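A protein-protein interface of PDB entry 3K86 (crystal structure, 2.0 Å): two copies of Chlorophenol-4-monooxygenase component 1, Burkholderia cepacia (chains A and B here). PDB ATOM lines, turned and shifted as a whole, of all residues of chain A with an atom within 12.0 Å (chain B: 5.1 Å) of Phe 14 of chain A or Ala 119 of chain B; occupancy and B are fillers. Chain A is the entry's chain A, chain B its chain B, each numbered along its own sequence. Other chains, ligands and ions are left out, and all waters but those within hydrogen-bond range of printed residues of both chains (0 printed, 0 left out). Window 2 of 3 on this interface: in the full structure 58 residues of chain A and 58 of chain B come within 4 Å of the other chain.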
ATOM      1  N   PHE A  14      14.356 -11.690 -18.863  1.00  0.00           N
ATOM      2  CA  PHE A  14      14.959 -13.022 -18.752  1.00  0.00           C
ATOM      3  C   PHE A  14      14.656 -13.673 -17.410  1.00  0.00           C
ATOM      4  O   PHE A  14      14.480 -12.981 -16.396  1.00  0.00           O
ATOM      5  CB  PHE A  14      16.483 -12.961 -18.958  1.00  0.00           C
ATOM      6  CG  PHE A  14      16.893 -12.483 -20.326  1.00  0.00           C
ATOM      7  CD1 PHE A  14      17.240 -11.158 -20.530  1.00  0.00           C
ATOM      8  CD2 PHE A  14      16.916 -13.354 -21.398  1.00  0.00           C
ATOM      9  CE1 PHE A  14      17.607 -10.705 -21.778  1.00  0.00           C
ATOM     10  CE2 PHE A  14      17.281 -12.912 -22.655  1.00  0.00           C
ATOM     11  CZ  PHE A  14      17.626 -11.579 -22.844  1.00  0.00           C
ATOM     12  N   GLU A  15      14.593 -15.005 -17.407  1.00  0.00           N
ATOM     13  CA  GLU A  15      14.560 -15.761 -16.158  1.00  0.00           C
ATOM     14  C   GLU A  15      15.990 -16.115 -15.688  1.00  0.00           C
ATOM     15  O   GLU A  15      16.843 -16.515 -16.483  1.00  0.00           O
ATOM     16  CB  GLU A  15      13.698 -17.027 -16.306  1.00  0.00           C
ATOM     17  CG  GLU A  15      12.213 -16.763 -16.607  1.00  0.00           C
ATOM     18  CD  GLU A  15      11.411 -18.054 -16.792  1.00  0.00           C
ATOM     19  OE1 GLU A  15      12.020 -19.151 -16.827  1.00  0.00           O
ATOM     20  OE2 GLU A  15      10.166 -17.970 -16.908  1.00  0.00           O
ATOM     21  N   THR A  16      16.244 -15.988 -14.392  1.00  0.00           N
ATOM     22  CA  THR A  16      17.567 -16.304 -13.857  1.00  0.00           C
ATOM     23  C   THR A  16      17.737 -17.834 -13.820  1.00  0.00           C
ATOM     24  O   THR A  16      16.748 -18.577 -13.767  1.00  0.00           O
ATOM     25  CB  THR A  16      17.807 -15.617 -12.461  1.00  0.00           C
ATOM     26  OG1 THR A  16      16.706 -15.879 -11.588  1.00  0.00           O
ATOM     27  CG2 THR A  16      17.954 -14.089 -12.597  1.00  0.00           C
ATOM     28  N   VAL A  17      18.973 -18.322 -13.891  1.00  0.00           N
ATOM     29  CA  VAL A  17      19.184 -19.769 -13.777  1.00  0.00           C
ATOM     30  C   VAL A  17      18.728 -20.242 -12.382  1.00  0.00           C
ATOM     31  O   VAL A  17      18.524 -19.424 -11.480  1.00  0.00           O
ATOM     32  CB  VAL A  17      20.663 -20.176 -14.005  1.00  0.00           C
ATOM     33  CG1 VAL A  17      21.105 -19.921 -15.469  1.00  0.00           C
ATOM     34  CG2 VAL A  17      21.557 -19.470 -13.014  1.00  0.00           C
ATOM     35  N   ALA A  18      18.559 -21.556 -12.220  1.00  0.00           N
ATOM     36  CA  ALA A  18      18.285 -22.168 -10.920  1.00  0.00           C
ATOM     37  C   ALA A  18      19.490 -21.990  -9.989  1.00  0.00           C
ATOM     38  O   ALA A  18      20.643 -22.059 -10.412  1.00  0.00           O
ATOM     39  CB  ALA A  18      17.947 -23.688 -11.087  1.00  0.00           C
ATOM     40  N   ASP A  21      21.869 -24.716 -10.206  1.00  0.00           N
ATOM     41  CA  ASP A  21      22.672 -24.689 -11.417  1.00  0.00           C
ATOM     42  C   ASP A  21      23.801 -23.680 -11.237  1.00  0.00           C
ATOM     43  O   ASP A  21      24.943 -23.940 -11.615  1.00  0.00           O
ATOM     44  CB  ASP A  21      21.765 -24.284 -12.582  1.00  0.00           C
ATOM     45  CG  ASP A  21      22.314 -24.700 -13.934  1.00  0.00           C
ATOM     46  OD1 ASP A  21      21.897 -24.082 -14.952  1.00  0.00           O
ATOM     47  OD2 ASP A  21      23.150 -25.640 -13.979  1.00  0.00           O
ATOM     48  N   THR B 117      26.374 -16.150 -28.867  1.00  0.00           N
ATOM     49  CA  THR B 117      25.360 -15.677 -27.929  1.00  0.00           C
ATOM     50  C   THR B 117      24.693 -16.881 -27.321  1.00  0.00           C
ATOM     51  O   THR B 117      24.738 -17.969 -27.889  1.00  0.00           O
ATOM     52  CB  THR B 117      24.268 -14.853 -28.590  1.00  0.00           C
ATOM     53  OG1 THR B 117      23.766 -15.579 -29.706  1.00  0.00           O
ATOM     54  CG2 THR B 117      24.814 -13.471 -29.038  1.00  0.00           C
ATOM     55  N   ILE B 118      24.067 -16.660 -26.168  1.00  0.00           N
ATOM     56  CA  ILE B 118      23.254 -17.661 -25.483  1.00  0.00           C
ATOM     57  C   ILE B 118      21.901 -17.074 -25.281  1.00  0.00           C
ATOM     58  O   ILE B 118      21.002 -17.427 -26.029  1.00  0.00           O
ATOM     59  CB  ILE B 118      23.857 -18.115 -24.165  1.00  0.00           C
ATOM     60  CG1 ILE B 118      25.243 -18.723 -24.427  1.00  0.00           C
ATOM     61  CG2 ILE B 118      22.937 -19.160 -23.487  1.00  0.00           C
ATOM     62  CD1 ILE B 118      25.971 -19.167 -23.122  1.00  0.00           C
ATOM     63  N   ALA B 119      21.743 -16.140 -24.327  1.00  0.00           N
ATOM     64  CA  ALA B 119      20.433 -15.579 -24.010  1.00  0.00           C
ATOM     65  C   ALA B 119      20.344 -14.067 -24.153  1.00  0.00           C
ATOM     66  O   ALA B 119      19.401 -13.586 -24.714  1.00  0.00           O
ATOM     67  CB  ALA B 119      19.973 -15.983 -22.603  1.00  0.00           C
ATOM     68  N   THR B 120      21.297 -13.311 -23.620  1.00  0.00           N
ATOM     69  CA  THR B 120      21.156 -11.864 -23.656  1.00  0.00           C
ATOM     70  C   THR B 120      21.574 -11.176 -24.930  1.00  0.00           C
ATOM     71  O   THR B 120      21.182 -10.059 -25.130  1.00  0.00           O
ATOM     72  CB  THR B 120      21.989 -11.175 -22.545  1.00  0.00           C
ATOM     73  OG1 THR B 120      23.382 -11.426 -22.791  1.00  0.00           O
ATOM     74  CG2 THR B 120      21.606 -11.736 -21.181  1.00  0.00           C
ATOM     75  N   GLY B 121      22.395 -11.815 -25.756  1.00  0.00           N
ATOM     76  CA  GLY B 121      23.091 -11.147 -26.842  1.00  0.00           C
ATOM     77  C   GLY B 121      24.584 -10.869 -26.526  1.00  0.00           C
ATOM     78  O   GLY B 121      25.393 -10.571 -27.427  1.00  0.00           O
ATOM     79  N   ASP B 133      26.039 -15.826 -18.671  1.00  0.00           N
ATOM     80  CA  ASP B 133      25.348 -14.796 -19.410  1.00  0.00           C
ATOM     81  C   ASP B 133      24.410 -14.014 -18.479  1.00  0.00           C
ATOM     82  O   ASP B 133      23.561 -14.620 -17.826  1.00  0.00           O
ATOM     83  CB  ASP B 133      24.519 -15.452 -20.547  1.00  0.00           C
ATOM     84  CG  ASP B 133      24.036 -14.432 -21.625  1.00  0.00           C
ATOM     85  OD1 ASP B 133      24.445 -13.254 -21.632  1.00  0.00           O
ATOM     86  OD2 ASP B 133      23.257 -14.787 -22.509  1.00  0.00           O
ATOM     87  N   THR B 135      22.338 -10.143 -16.970  1.00  0.00           N
ATOM     88  CA  THR B 135      21.779  -8.796 -17.090  1.00  0.00           C
ATOM     89  C   THR B 135      22.249  -7.954 -15.909  1.00  0.00           C
ATOM     90  O   THR B 135      22.255  -8.415 -14.736  1.00  0.00           O
ATOM     91  CB  THR B 135      20.222  -8.821 -17.119  1.00  0.00           C
ATOM     92  OG1 THR B 135      19.757  -9.398 -15.891  1.00  0.00           O
ATOM     93  CG2 THR B 135      19.762  -9.773 -18.243  1.00  0.00           C
ATOM     94  N   VAL B 153      21.531 -15.337 -16.171  1.00  0.00           N
ATOM     95  CA  VAL B 153      20.322 -15.819 -16.847  1.00  0.00           C
ATOM     96  C   VAL B 153      20.603 -17.098 -17.661  1.00  0.00           C
ATOM     97  O   VAL B 153      19.684 -17.800 -18.046  1.00  0.00           O
ATOM     98  CB  VAL B 153      19.673 -14.735 -17.742  1.00  0.00           C
ATOM     99  CG1 VAL B 153      19.171 -13.553 -16.885  1.00  0.00           C
ATOM    100  CG2 VAL B 153      20.619 -14.240 -18.712  1.00  0.00           C
ATOM    101  N   ALA B 154      21.869 -17.383 -17.923  1.00  0.00           N
ATOM    102  CA  ALA B 154      22.264 -18.630 -18.600  1.00  0.00           C
ATOM    103  C   ALA B 154      23.703 -18.918 -18.325  1.00  0.00           C
ATOM    104  O   ALA B 154      24.480 -18.019 -17.936  1.00  0.00           O
ATOM    105  CB  ALA B 154      22.042 -18.548 -20.132  1.00  0.00           C
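The backbone carbonyl oxygen (O) of Glu 15 of chain A lies close to the backbone carbonyl oxygen (O) of Val 153 of chain B (3.5 Å).
OD2 of Asp 133 of chain B is in hydrogen-bond range of N of Ala 119 of chain B.
OD1 of Asp 133 of chain B is in hydrogen-bond range of OG1 of Thr 120 of chain B (2.4 Å).
N of Val 153 of chain B sits at hydrogen-bond distance from O of Asp 133 of chain B (2.7 Å).
The backbone NH of Asp 133 of chain B sits at hydrogen-bond distance from the backbone carbonyl oxygen of Ala 154 of chain B.
Among the printed residues, pairs that only touch across the chains: Phe 14 of chain A with Ala 119 of chain B (3.0 Å), Phe 14 of chain A with Thr 120 of chain B (3.6 Å), Phe 14 of chain A with Thr 135 of chain B (3.7 Å), Phe 14 of chain A with Val 153 of chain B (3.4 Å), Val 17 of chain A with Val 153 of chain B (3.6 Å) and Val 17 of chain A with Ala 154 of chain B (3.6 Å).
Phe 14 of chain A touches just these residues of chain B: Ala 119 (3.0 Å), Thr 120 (3.6 Å), Thr 135 (3.7 Å) and Val 153 (3.4 Å).
Ala 119 of chain B touches just one residue of chain A: Phe 14.
No residue of chain A comes within 4 Å of Thr 117 of chain B.
No residue of chain A comes within 4 Å of Gly 121 of chain B.
Asp 133 of chain B touches none of the printed residues of chain A.
Of chain A, only Phe 14, Glu 15 and Val 17 come within 4 Å of Val 153 of chain B.
Ala 154 of chain B touches just one residue of chain A: Val 17.
Of the printed residues of chain B, Val 17 of chain A touches Val 153 and Ala 154.
Of the printed residues of chain B, Glu 15 of chain A touches Val 153.
Printed residues of chain A within 4 Å of Thr 135 of chain B: Phe 14 (3.7 Å).
Asp 21 of chain A touches none of the printed residues of chain B.
Ala 18 of chain A touches none of the printed residues of chain B.
The nearest printed residue of chain B that does not touch Phe 14 of chain A is Gly 121 of chain B (5.6 Å).
Of the 9 printed residues of chain B, 5 touch a printed residue of chain A.
Of the 6 printed residues of chain A, 3 touch a printed residue of chain B.
No position is printed for both chains.
Of the 7 pairs that touch across the chains among the printed residues, none has its exchanged pair printed and touching as well.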
